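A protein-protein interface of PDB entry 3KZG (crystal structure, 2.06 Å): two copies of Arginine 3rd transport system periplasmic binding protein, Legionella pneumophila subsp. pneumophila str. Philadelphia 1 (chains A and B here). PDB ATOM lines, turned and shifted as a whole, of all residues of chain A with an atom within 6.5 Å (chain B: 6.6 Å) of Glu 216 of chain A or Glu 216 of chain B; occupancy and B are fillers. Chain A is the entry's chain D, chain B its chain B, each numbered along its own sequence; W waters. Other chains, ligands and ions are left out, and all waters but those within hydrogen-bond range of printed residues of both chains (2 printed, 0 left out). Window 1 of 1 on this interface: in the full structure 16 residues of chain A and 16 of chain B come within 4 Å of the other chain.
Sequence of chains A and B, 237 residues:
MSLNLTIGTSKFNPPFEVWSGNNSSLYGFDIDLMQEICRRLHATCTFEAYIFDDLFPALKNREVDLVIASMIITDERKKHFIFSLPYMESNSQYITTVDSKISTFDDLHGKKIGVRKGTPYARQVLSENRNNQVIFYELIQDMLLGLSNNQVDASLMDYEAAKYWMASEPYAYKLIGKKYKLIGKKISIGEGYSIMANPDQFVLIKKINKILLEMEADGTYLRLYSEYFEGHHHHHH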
ATOM      1  N   LEU A  85      32.974  29.432  22.229  1.00  0.00           N
ATOM      2  CA  LEU A  85      32.924  29.790  20.825  1.00  0.00           C
ATOM      3  C   LEU A  85      31.466  30.180  20.613  1.00  0.00           C
ATOM      4  O   LEU A  85      30.583  29.624  21.262  1.00  0.00           O
ATOM      5  CB  LEU A  85      33.235  28.580  19.937  1.00  0.00           C
ATOM      6  CG  LEU A  85      34.605  27.908  20.023  1.00  0.00           C
ATOM      7  CD1 LEU A  85      34.641  26.702  19.093  1.00  0.00           C
ATOM      8  CD2 LEU A  85      35.690  28.908  19.640  1.00  0.00           C
ATOM      9  N   PRO A  86      31.192  31.142  19.716  1.00  0.00           N
ATOM     10  CA  PRO A  86      29.794  31.519  19.500  1.00  0.00           C
ATOM     11  C   PRO A  86      29.039  30.387  18.814  1.00  0.00           C
ATOM     12  O   PRO A  86      29.593  29.712  17.947  1.00  0.00           O
ATOM     13  CB  PRO A  86      29.900  32.774  18.627  1.00  0.00           C
ATOM     14  CG  PRO A  86      31.177  32.543  17.854  1.00  0.00           C
ATOM     15  CD  PRO A  86      32.103  31.980  18.917  1.00  0.00           C
ATOM     16  N   TYR A  87      27.786  30.158  19.212  1.00  0.00           N
ATOM     17  CA  TYR A  87      27.002  29.103  18.592  1.00  0.00           C
ATOM     18  C   TYR A  87      26.117  29.645  17.474  1.00  0.00           C
ATOM     19  O   TYR A  87      25.351  28.908  16.865  1.00  0.00           O
ATOM     20  CB  TYR A  87      26.166  28.345  19.635  1.00  0.00           C
ATOM     21  CG  TYR A  87      25.302  29.201  20.541  1.00  0.00           C
ATOM     22  CD1 TYR A  87      24.068  29.695  20.113  1.00  0.00           C
ATOM     23  CD2 TYR A  87      25.702  29.469  21.850  1.00  0.00           C
ATOM     24  CE1 TYR A  87      23.245  30.423  20.980  1.00  0.00           C
ATOM     25  CE2 TYR A  87      24.894  30.198  22.720  1.00  0.00           C
ATOM     26  CZ  TYR A  87      23.665  30.669  22.282  1.00  0.00           C
ATOM     27  OH  TYR A  87      22.859  31.364  23.156  1.00  0.00           O
ATOM     28  N   ASN A 209      33.893  24.050  23.989  1.00  0.00           N
ATOM     29  CA  ASN A 209      34.241  24.451  22.625  1.00  0.00           C
ATOM     30  C   ASN A 209      34.500  23.248  21.730  1.00  0.00           C
ATOM     31  O   ASN A 209      34.148  23.256  20.550  1.00  0.00           O
ATOM     32  CB  ASN A 209      35.465  25.367  22.625  1.00  0.00           C
ATOM     33  CG  ASN A 209      35.169  26.728  23.240  1.00  0.00           C
ATOM     34  OD1 ASN A 209      34.018  27.166  23.263  1.00  0.00           O
ATOM     35  ND2 ASN A 209      36.200  27.404  23.722  1.00  0.00           N
ATOM     36  N   ILE A 211      33.137  20.308  22.102  1.00  0.00           N
ATOM     37  CA  ILE A 211      31.855  19.639  21.875  1.00  0.00           C
ATOM     38  C   ILE A 211      31.086  20.392  20.782  1.00  0.00           C
ATOM     39  O   ILE A 211      30.411  19.780  19.953  1.00  0.00           O
ATOM     40  CB  ILE A 211      30.993  19.590  23.177  1.00  0.00           C
ATOM     41  CG1 ILE A 211      31.682  18.726  24.246  1.00  0.00           C
ATOM     42  CG2 ILE A 211      29.597  19.059  22.869  1.00  0.00           C
ATOM     43  CD1 ILE A 211      31.980  17.295  23.804  1.00  0.00           C
ATOM     44  N   LEU A 212      31.191  21.719  20.778  1.00  0.00           N
ATOM     45  CA  LEU A 212      30.509  22.515  19.767  1.00  0.00           C
ATOM     46  C   LEU A 212      31.070  22.143  18.401  1.00  0.00           C
ATOM     47  O   LEU A 212      30.315  21.949  17.447  1.00  0.00           O
ATOM     48  CB  LEU A 212      30.692  24.016  20.034  1.00  0.00           C
ATOM     49  CG  LEU A 212      29.782  24.621  21.101  1.00  0.00           C
ATOM     50  CD1 LEU A 212      30.198  26.052  21.421  1.00  0.00           C
ATOM     51  CD2 LEU A 212      28.336  24.570  20.582  1.00  0.00           C
ATOM     52  N   LEU A 213      32.395  22.026  18.316  1.00  0.00           N
ATOM     53  CA  LEU A 213      33.043  21.656  17.060  1.00  0.00           C
ATOM     54  C   LEU A 213      32.619  20.260  16.610  1.00  0.00           C
ATOM     55  O   LEU A 213      32.406  20.022  15.423  1.00  0.00           O
ATOM     56  CB  LEU A 213      34.566  21.709  17.205  1.00  0.00           C
ATOM     57  CG  LEU A 213      35.181  23.100  17.363  1.00  0.00           C
ATOM     58  CD1 LEU A 213      36.680  22.976  17.608  1.00  0.00           C
ATOM     59  CD2 LEU A 213      34.908  23.923  16.100  1.00  0.00           C
ATOM     60  N   GLU A 214      32.495  19.337  17.556  1.00  0.00           N
ATOM     61  CA  GLU A 214      32.085  17.978  17.224  1.00  0.00           C
ATOM     62  C   GLU A 214      30.626  17.962  16.767  1.00  0.00           C
ATOM     63  O   GLU A 214      30.258  17.211  15.864  1.00  0.00           O
ATOM     64  CB  GLU A 214      32.295  17.059  18.439  1.00  0.00           C
ATOM     65  CG  GLU A 214      33.747  17.054  18.928  1.00  0.00           C
ATOM     66  CD  GLU A 214      33.952  16.355  20.266  1.00  0.00           C
ATOM     67  OE1 GLU A 214      32.963  16.130  20.998  1.00  0.00           O
ATOM     68  OE2 GLU A 214      35.118  16.048  20.600  1.00  0.00           O
ATOM     69  N   MET A 215      29.790  18.796  17.378  1.00  0.00           N
ATOM     70  CA  MET A 215      28.387  18.845  16.982  1.00  0.00           C
ATOM     71  C   MET A 215      28.262  19.405  15.566  1.00  0.00           C
ATOM     72  O   MET A 215      27.408  18.968  14.790  1.00  0.00           O
ATOM     73  CB  MET A 215      27.574  19.708  17.950  1.00  0.00           C
ATOM     74  CG  MET A 215      27.294  19.049  19.308  1.00  0.00           C
ATOM     75  SD  MET A 215      26.493  20.256  20.513  1.00  0.00           S
ATOM     76  CE  MET A 215      24.812  20.547  19.609  1.00  0.00           C
ATOM     77  N   GLU A 216      29.120  20.366  15.231  1.00  0.00           N
ATOM     78  CA  GLU A 216      29.093  20.978  13.908  1.00  0.00           C
ATOM     79  C   GLU A 216      29.647  20.018  12.868  1.00  0.00           C
ATOM     80  O   GLU A 216      29.225  20.032  11.710  1.00  0.00           O
ATOM     81  CB  GLU A 216      29.899  22.285  13.909  1.00  0.00           C
ATOM     82  CG  GLU A 216      29.452  23.234  15.006  1.00  0.00           C
ATOM     83  CD  GLU A 216      30.149  24.580  14.982  1.00  0.00           C
ATOM     84  OE1 GLU A 216      31.396  24.615  14.926  1.00  0.00           O
ATOM     85  OE2 GLU A 216      29.437  25.606  15.038  1.00  0.00           O
ATOM     86  N   ALA A 217      30.589  19.178  13.285  1.00  0.00           N
ATOM     87  CA  ALA A 217      31.197  18.210  12.382  1.00  0.00           C
ATOM     88  C   ALA A 217      30.276  17.040  12.029  1.00  0.00           C
ATOM     89  O   ALA A 217      30.328  16.536  10.909  1.00  0.00           O
ATOM     90  CB  ALA A 217      32.497  17.673  12.982  1.00  0.00           C
ATOM     91  N   ASP A 218      29.432  16.610  12.965  1.00  0.00           N
ATOM     92  CA  ASP A 218      28.564  15.467  12.679  1.00  0.00           C
ATOM     93  C   ASP A 218      27.132  15.773  12.259  1.00  0.00           C
ATOM     94  O   ASP A 218      26.318  14.855  12.117  1.00  0.00           O
ATOM     95  CB  ASP A 218      28.553  14.482  13.859  1.00  0.00           C
ATOM     96  CG  ASP A 218      27.907  15.053  15.108  1.00  0.00           C
ATOM     97  OD1 ASP A 218      27.132  16.036  15.012  1.00  0.00           O
ATOM     98  OD2 ASP A 218      28.165  14.492  16.197  1.00  0.00           O
ATOM     99  N   GLY A 219      26.823  17.052  12.064  1.00  0.00           N
ATOM    100  CA  GLY A 219      25.487  17.436  11.634  1.00  0.00           C
ATOM    101  C   GLY A 219      24.469  17.750  12.717  1.00  0.00           C
ATOM    102  O   GLY A 219      23.391  18.270  12.418  1.00  0.00           O
ATOM    103  N   THR A 220      24.800  17.444  13.969  1.00  0.00           N
ATOM    104  CA  THR A 220      23.891  17.693  15.085  1.00  0.00           C
ATOM    105  C   THR A 220      23.525  19.165  15.258  1.00  0.00           C
ATOM    106  O   THR A 220      22.366  19.499  15.533  1.00  0.00           O
ATOM    107  CB  THR A 220      24.491  17.181  16.405  1.00  0.00           C
ATOM    108  OG1 THR A 220      24.658  15.761  16.324  1.00  0.00           O
ATOM    109  CG2 THR A 220      23.583  17.523  17.583  1.00  0.00           C
ATOM    110  N   TYR A 221      24.514  20.041  15.102  1.00  0.00           N
ATOM    111  CA  TYR A 221      24.291  21.477  15.237  1.00  0.00           C
ATOM    112  C   TYR A 221      23.375  21.999  14.137  1.00  0.00           C
ATOM    113  O   TYR A 221      22.413  22.715  14.403  1.00  0.00           O
ATOM    114  CB  TYR A 221      25.628  22.237  15.201  1.00  0.00           C
ATOM    115  CG  TYR A 221      25.460  23.737  15.039  1.00  0.00           C
ATOM    116  CD1 TYR A 221      25.439  24.326  13.773  1.00  0.00           C
ATOM    117  CD2 TYR A 221      25.255  24.556  16.147  1.00  0.00           C
ATOM    118  CE1 TYR A 221      25.214  25.696  13.612  1.00  0.00           C
ATOM    119  CE2 TYR A 221      25.023  25.932  16.000  1.00  0.00           C
ATOM    120  CZ  TYR A 221      25.005  26.491  14.728  1.00  0.00           C
ATOM    121  OH  TYR A 221      24.767  27.836  14.574  1.00  0.00           O
ATOM    122  N   LEU A 222      23.682  21.649  12.898  1.00  0.00           N
ATOM    123  CA  LEU A 222      22.864  22.100  11.778  1.00  0.00           C
ATOM    124  C   LEU A 222      21.401  21.671  11.964  1.00  0.00           C
ATOM    125  O   LEU A 222      20.476  22.457  11.747  1.00  0.00           O
ATOM    126  CB  LEU A 222      23.425  21.536  10.473  1.00  0.00           C
ATOM    127  CG  LEU A 222      22.723  21.974   9.185  1.00  0.00           C
ATOM    128  CD1 LEU A 222      22.684  23.491   9.097  1.00  0.00           C
ATOM    129  CD2 LEU A 222      23.446  21.365   7.998  1.00  0.00           C
ATOM    130  N   TYR A 225      19.828  23.830  14.686  1.00  0.00           N
ATOM    131  CA  TYR A 225      19.715  25.198  14.178  1.00  0.00           C
ATOM    132  C   TYR A 225      18.559  25.340  13.190  1.00  0.00           C
ATOM    133  O   TYR A 225      17.766  26.283  13.275  1.00  0.00           O
ATOM    134  CB  TYR A 225      21.019  25.620  13.484  1.00  0.00           C
ATOM    135  CG  TYR A 225      20.988  27.014  12.880  1.00  0.00           C
ATOM    136  CD1 TYR A 225      21.338  28.133  13.633  1.00  0.00           C
ATOM    137  CD2 TYR A 225      20.595  27.210  11.558  1.00  0.00           C
ATOM    138  CE1 TYR A 225      21.301  29.419  13.082  1.00  0.00           C
ATOM    139  CE2 TYR A 225      20.553  28.489  11.000  1.00  0.00           C
ATOM    140  CZ  TYR A 225      20.908  29.586  11.769  1.00  0.00           C
ATOM    141  OH  TYR A 225      20.863  30.846  11.212  1.00  0.00           O
ATOM    142  N   ARG B  40      32.880  34.708  -0.077  1.00  0.00           N
ATOM    143  CA  ARG B  40      31.992  35.405   0.840  1.00  0.00           C
ATOM    144  C   ARG B  40      32.530  36.741   1.325  1.00  0.00           C
ATOM    145  O   ARG B  40      31.751  37.612   1.704  1.00  0.00           O
ATOM    146  CB  ARG B  40      31.621  34.491   2.014  1.00  0.00           C
ATOM    147  CG  ARG B  40      30.732  33.319   1.566  1.00  0.00           C
ATOM    148  CD  ARG B  40      30.432  32.331   2.689  1.00  0.00           C
ATOM    149  NE  ARG B  40      29.634  31.202   2.212  1.00  0.00           N
ATOM    150  CZ  ARG B  40      28.404  30.915   2.636  1.00  0.00           C
ATOM    151  NH1 ARG B  40      27.811  31.670   3.555  1.00  0.00           N
ATOM    152  NH2 ARG B  40      27.762  29.868   2.136  1.00  0.00           N
ATOM    153  N   LEU B  85      37.808  31.866  14.401  1.00  0.00           N
ATOM    154  CA  LEU B  85      37.150  30.821  15.165  1.00  0.00           C
ATOM    155  C   LEU B  85      37.696  29.529  14.552  1.00  0.00           C
ATOM    156  O   LEU B  85      37.960  29.482  13.350  1.00  0.00           O
ATOM    157  CB  LEU B  85      35.633  30.878  14.950  1.00  0.00           C
ATOM    158  CG  LEU B  85      34.815  32.099  15.383  1.00  0.00           C
ATOM    159  CD1 LEU B  85      33.364  31.895  14.932  1.00  0.00           C
ATOM    160  CD2 LEU B  85      34.886  32.289  16.888  1.00  0.00           C
ATOM    161  N   PRO B  86      37.907  28.478  15.364  1.00  0.00           N
ATOM    162  CA  PRO B  86      38.417  27.234  14.782  1.00  0.00           C
ATOM    163  C   PRO B  86      37.373  26.624  13.839  1.00  0.00           C
ATOM    164  O   PRO B  86      36.177  26.747  14.078  1.00  0.00           O
ATOM    165  CB  PRO B  86      38.687  26.360  16.011  1.00  0.00           C
ATOM    166  CG  PRO B  86      37.706  26.877  17.028  1.00  0.00           C
ATOM    167  CD  PRO B  86      37.805  28.370  16.832  1.00  0.00           C
ATOM    168  N   TYR B  87      37.822  25.976  12.769  1.00  0.00           N
ATOM    169  CA  TYR B  87      36.903  25.371  11.801  1.00  0.00           C
ATOM    170  C   TYR B  87      36.858  23.863  11.942  1.00  0.00           C
ATOM    171  O   TYR B  87      36.163  23.167  11.192  1.00  0.00           O
ATOM    172  CB  TYR B  87      37.306  25.746  10.363  1.00  0.00           C
ATOM    173  CG  TYR B  87      38.734  25.406   9.970  1.00  0.00           C
ATOM    174  CD1 TYR B  87      39.076  24.127   9.528  1.00  0.00           C
ATOM    175  CD2 TYR B  87      39.740  26.372  10.026  1.00  0.00           C
ATOM    176  CE1 TYR B  87      40.385  23.821   9.153  1.00  0.00           C
ATOM    177  CE2 TYR B  87      41.054  26.079   9.652  1.00  0.00           C
ATOM    178  CZ  TYR B  87      41.367  24.804   9.219  1.00  0.00           C
ATOM    179  OH  TYR B  87      42.660  24.496   8.867  1.00  0.00           O
ATOM    180  N   ASN B 209      35.200  35.296  10.991  1.00  0.00           N
ATOM    181  CA  ASN B 209      34.447  34.593  12.031  1.00  0.00           C
ATOM    182  C   ASN B 209      32.940  34.616  11.735  1.00  0.00           C
ATOM    183  O   ASN B 209      32.244  33.614  11.919  1.00  0.00           O
ATOM    184  CB  ASN B 209      34.733  35.227  13.405  1.00  0.00           C
ATOM    185  CG  ASN B 209      36.151  34.936  13.904  1.00  0.00           C
ATOM    186  OD1 ASN B 209      36.806  34.022  13.417  1.00  0.00           O
ATOM    187  ND2 ASN B 209      36.614  35.704  14.893  1.00  0.00           N
ATOM    188  N   ILE B 211      31.628  34.882   8.802  1.00  0.00           N
ATOM    189  CA  ILE B 211      31.470  34.043   7.621  1.00  0.00           C
ATOM    190  C   ILE B 211      31.455  32.551   7.975  1.00  0.00           C
ATOM    191  O   ILE B 211      30.718  31.768   7.375  1.00  0.00           O
ATOM    192  CB  ILE B 211      32.593  34.333   6.582  1.00  0.00           C
ATOM    193  CG1 ILE B 211      32.335  35.678   5.899  1.00  0.00           C
ATOM    194  CG2 ILE B 211      32.656  33.236   5.543  1.00  0.00           C
ATOM    195  CD1 ILE B 211      33.429  36.098   4.925  1.00  0.00           C
ATOM    196  N   LEU B 212      32.277  32.161   8.940  1.00  0.00           N
ATOM    197  CA  LEU B 212      32.320  30.772   9.379  1.00  0.00           C
ATOM    198  C   LEU B 212      30.969  30.449  10.026  1.00  0.00           C
ATOM    199  O   LEU B 212      30.352  29.434   9.718  1.00  0.00           O
ATOM    200  CB  LEU B 212      33.469  30.562  10.381  1.00  0.00           C
ATOM    201  CG  LEU B 212      34.868  30.544   9.752  1.00  0.00           C
ATOM    202  CD1 LEU B 212      35.943  30.600  10.823  1.00  0.00           C
ATOM    203  CD2 LEU B 212      35.015  29.286   8.902  1.00  0.00           C
ATOM    204  N   LEU B 213      30.496  31.327  10.899  1.00  0.00           N
ATOM    205  CA  LEU B 213      29.208  31.095  11.548  1.00  0.00           C
ATOM    206  C   LEU B 213      28.108  30.959  10.499  1.00  0.00           C
ATOM    207  O   LEU B 213      27.240  30.103  10.619  1.00  0.00           O
ATOM    208  CB  LEU B 213      28.866  32.236  12.507  1.00  0.00           C
ATOM    209  CG  LEU B 213      29.685  32.316  13.798  1.00  0.00           C
ATOM    210  CD1 LEU B 213      29.171  33.468  14.652  1.00  0.00           C
ATOM    211  CD2 LEU B 213      29.581  30.999  14.567  1.00  0.00           C
ATOM    212  N   GLU B 214      28.162  31.800   9.469  1.00  0.00           N
ATOM    213  CA  GLU B 214      27.169  31.773   8.401  1.00  0.00           C
ATOM    214  C   GLU B 214      27.252  30.487   7.599  1.00  0.00           C
ATOM    215  O   GLU B 214      26.227  29.926   7.215  1.00  0.00           O
ATOM    216  CB  GLU B 214      27.336  33.002   7.501  1.00  0.00           C
ATOM    217  CG  GLU B 214      27.032  34.278   8.274  1.00  0.00           C
ATOM    218  CD  GLU B 214      27.317  35.565   7.518  1.00  0.00           C
ATOM    219  OE1 GLU B 214      28.070  35.544   6.524  1.00  0.00           O
ATOM    220  OE2 GLU B 214      26.793  36.615   7.947  1.00  0.00           O
ATOM    221  N   MET B 215      28.469  30.010   7.354  1.00  0.00           N
ATOM    222  CA  MET B 215      28.655  28.760   6.617  1.00  0.00           C
ATOM    223  C   MET B 215      28.116  27.579   7.414  1.00  0.00           C
ATOM    224  O   MET B 215      27.616  26.602   6.855  1.00  0.00           O
ATOM    225  CB  MET B 215      30.137  28.520   6.311  1.00  0.00           C
ATOM    226  CG  MET B 215      30.684  29.396   5.190  1.00  0.00           C
ATOM    227  SD  MET B 215      32.546  29.236   4.957  1.00  0.00           S
ATOM    228  CE  MET B 215      32.560  27.486   4.223  1.00  0.00           C
ATOM    229  N   GLU B 216      28.233  27.669   8.731  1.00  0.00           N
ATOM    230  CA  GLU B 216      27.763  26.606   9.600  1.00  0.00           C
ATOM    231  C   GLU B 216      26.240  26.623   9.683  1.00  0.00           C
ATOM    232  O   GLU B 216      25.605  25.587   9.869  1.00  0.00           O
ATOM    233  CB  GLU B 216      28.394  26.767  10.987  1.00  0.00           C
ATOM    234  CG  GLU B 216      29.900  26.925  10.887  1.00  0.00           C
ATOM    235  CD  GLU B 216      30.622  26.825  12.206  1.00  0.00           C
ATOM    236  OE1 GLU B 216      30.280  27.575  13.145  1.00  0.00           O
ATOM    237  OE2 GLU B 216      31.551  25.995  12.293  1.00  0.00           O
ATOM    238  N   ALA B 217      25.657  27.804   9.521  1.00  0.00           N
ATOM    239  CA  ALA B 217      24.207  27.946   9.590  1.00  0.00           C
ATOM    240  C   ALA B 217      23.476  27.509   8.320  1.00  0.00           C
ATOM    241  O   ALA B 217      22.341  27.033   8.397  1.00  0.00           O
ATOM    242  CB  ALA B 217      23.840  29.395   9.925  1.00  0.00           C
ATOM    243  N   ASP B 218      24.112  27.661   7.157  1.00  0.00           N
ATOM    244  CA  ASP B 218      23.460  27.292   5.901  1.00  0.00           C
ATOM    245  C   ASP B 218      23.833  25.931   5.312  1.00  0.00           C
ATOM    246  O   ASP B 218      23.384  25.590   4.224  1.00  0.00           O
ATOM    247  CB  ASP B 218      23.679  28.385   4.843  1.00  0.00           C
ATOM    248  CG  ASP B 218      25.127  28.505   4.403  1.00  0.00           C
ATOM    249  OD1 ASP B 218      25.910  27.556   4.615  1.00  0.00           O
ATOM    250  OD2 ASP B 218      25.476  29.552   3.822  1.00  0.00           O
ATOM    251  N   GLY B 219      24.650  25.161   6.022  1.00  0.00           N
ATOM    252  CA  GLY B 219      25.018  23.839   5.533  1.00  0.00           C
ATOM    253  C   GLY B 219      26.255  23.751   4.661  1.00  0.00           C
ATOM    254  O   GLY B 219      26.711  22.657   4.329  1.00  0.00           O
ATOM    255  N   THR B 220      26.806  24.898   4.282  1.00  0.00           N
ATOM    256  CA  THR B 220      27.996  24.909   3.441  1.00  0.00           C
ATOM    257  C   THR B 220      29.155  24.223   4.150  1.00  0.00           C
ATOM    258  O   THR B 220      29.862  23.404   3.562  1.00  0.00           O
ATOM    259  CB  THR B 220      28.414  26.346   3.080  1.00  0.00           C
ATOM    260  OG1 THR B 220      27.382  26.968   2.297  1.00  0.00           O
ATOM    261  CG2 THR B 220      29.709  26.333   2.291  1.00  0.00           C
ATOM    262  N   TYR B 221      29.357  24.558   5.417  1.00  0.00           N
ATOM    263  CA  TYR B 221      30.448  23.952   6.163  1.00  0.00           C
ATOM    264  C   TYR B 221      30.302  22.435   6.230  1.00  0.00           C
ATOM    265  O   TYR B 221      31.224  21.696   5.856  1.00  0.00           O
ATOM    266  CB  TYR B 221      30.516  24.534   7.573  1.00  0.00           C
ATOM    267  CG  TYR B 221      31.470  23.793   8.471  1.00  0.00           C
ATOM    268  CD1 TYR B 221      31.029  22.725   9.260  1.00  0.00           C
ATOM    269  CD2 TYR B 221      32.828  24.122   8.498  1.00  0.00           C
ATOM    270  CE1 TYR B 221      31.921  22.006  10.051  1.00  0.00           C
ATOM    271  CE2 TYR B 221      33.724  23.403   9.282  1.00  0.00           C
ATOM    272  CZ  TYR B 221      33.264  22.351  10.054  1.00  0.00           C
ATOM    273  OH  TYR B 221      34.149  21.646  10.838  1.00  0.00           O
ATOM    274  N   LEU B 222      29.144  21.976   6.695  1.00  0.00           N
ATOM    275  CA  LEU B 222      28.877  20.546   6.821  1.00  0.00           C
ATOM    276  C   LEU B 222      29.087  19.798   5.504  1.00  0.00           C
ATOM    277  O   LEU B 222      29.674  18.716   5.479  1.00  0.00           O
ATOM    278  CB  LEU B 222      27.452  20.318   7.328  1.00  0.00           C
ATOM    279  CG  LEU B 222      27.064  18.866   7.601  1.00  0.00           C
ATOM    280  CD1 LEU B 222      27.934  18.294   8.722  1.00  0.00           C
ATOM    281  CD2 LEU B 222      25.596  18.799   7.972  1.00  0.00           C
ATOM    282  N   TYR B 225      32.826  19.653   4.881  1.00  0.00           N
ATOM    283  CA  TYR B 225      33.434  18.780   5.881  1.00  0.00           C
ATOM    284  C   TYR B 225      33.168  17.299   5.614  1.00  0.00           C
ATOM    285  O   TYR B 225      34.091  16.479   5.580  1.00  0.00           O
ATOM    286  CB  TYR B 225      32.914  19.135   7.277  1.00  0.00           C
ATOM    287  CG  TYR B 225      33.540  18.316   8.385  1.00  0.00           C
ATOM    288  CD1 TYR B 225      34.667  18.773   9.067  1.00  0.00           C
ATOM    289  CD2 TYR B 225      33.023  17.070   8.731  1.00  0.00           C
ATOM    290  CE1 TYR B 225      35.261  18.006  10.068  1.00  0.00           C
ATOM    291  CE2 TYR B 225      33.613  16.294   9.730  1.00  0.00           C
ATOM    292  CZ  TYR B 225      34.730  16.769  10.390  1.00  0.00           C
ATOM    293  OH  TYR B 225      35.330  16.000  11.361  1.00  0.00           O
HETATM  294  O   HOH W   1      25.759  29.840  12.991  1.00  0.00           O
HETATM  295  O   HOH W   2      34.123  20.971  13.564  1.00  0.00           O
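Water W2 bridges the backbone carbonyl oxygen of Leu 213 of chain A (2.7 Å) and the side-chain hydroxyl of Tyr 221 of chain B (2.8 Å). Water W1 bridges OH of Tyr 221 of chain A (2.7 Å) and O of Leu 213 of chain B (2.8 Å).
The side-chain carboxylate (OE2) of Glu 216 of chain A lies close to the side-chain carboxylate (OE1) of Glu 216 of chain B, at 2.9 Å.
Pro 86 of chain A touches Leu 213 of chain B, and with the chains exchanged Leu 213 of chain A touches Pro 86 of chain B. Glu 216 of chain A touches Tyr 221 of chain B, and with the chains exchanged Tyr 221 of chain A touches Glu 216 of chain B. Glu 216 of chain A touches Leu 222 of chain B, and with the chains exchanged Leu 222 of chain A touches Glu 216 of chain B. Ala 217 of chain A touches Tyr 225 of chain B, and with the chains exchanged Tyr 225 of chain A touches Ala 217 of chain B.
Among the printed residues, merely in contact across the chains: Leu 85 of chain A with Pro 86 of chain B (3.6 Å), Pro 86 of chain A with Leu 85 of chain B (3.5 Å), Pro 86 of chain A with Leu 213 of chain B (3.6 Å), Leu 213 of chain A with Pro 86 of chain B (3.7 Å), Glu 216 of chain A with Tyr 221 of chain B (3.7 Å), Glu 216 of chain A with Leu 222 of chain B (3.7 Å), Ala 217 of chain A with Leu 222 of chain B (3.7 Å), Ala 217 of chain A with Tyr 225 of chain B (3.5 Å), Gly 219 of chain A with Leu 222 of chain B (3.7 Å), Tyr 221 of chain A with Glu 216 of chain B (3.8 Å), Leu 222 of chain A with Glu 216 of chain B (3.7 Å), Leu 222 of chain A with Ala 217 of chain B (3.6 Å), Leu 222 of chain A with Gly 219 of chain B (3.8 Å), Leu 222 of chain A with Leu 222 of chain B (3.3 Å) and Tyr 225 of chain A with Ala 217 of chain B (3.5 Å).
The backbone NH (N) of Leu 85 of chain B is in hydrogen-bond range of the side-chain amide oxygen (OD1) of Asn 209 of chain B (2.6 Å). O of Tyr 87 of chain B sits at hydrogen-bond distance from OH of Tyr 221 of chain B. The backbone carbonyl oxygen (O) of Met 215 of chain B sits at hydrogen-bond distance from the backbone NH (N) of Tyr 221 of chain B (3.0 Å). OH of Tyr 221 of chain A lies within hydrogen-bond range of O of Tyr 87 of chain A (2.6 Å). The side-chain amide oxygen (OD1) of Asn 209 of chain A is in hydrogen-bond range of the backbone NH (N) of Leu 85 of chain A (2.7 Å). The backbone carbonyl oxygen (O) of Met 215 of chain A sits at hydrogen-bond distance from the backbone NH (N) of Tyr 221 of chain A, at 3.1 Å.
Of the 18 printed residues of chain B, 9 touch a printed residue of chain A. Of the 17 printed residues of chain A, 9 touch a printed residue of chain B. Hydrophobic or aromatic side chains of chain A within 4 Å of the printed part of chain B: Leu 85, Pro 86, Leu 213, Ala 217, Tyr 221, Leu 222 and Tyr 225.
Printed residues of chain B within 4 Å of Pro 86 of chain A: Leu 85 (3.5 Å) and Leu 213 (3.6 Å). Of the printed residues of chain B, Leu 213 of chain A touches Pro 86 (3.7 Å). Glu 216 of chain B touches three residues of chain A. Of the printed residues of chain A, Tyr 221 of chain B touches Glu 216 (3.7 Å). The nearest residue of chain B that does not touch Glu 216 of chain A is Pro 86 of chain B (5.3 Å). The nearest printed residue of chain B that does not touch Pro 86 of chain A is Glu 216 of chain B (5.3 Å).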
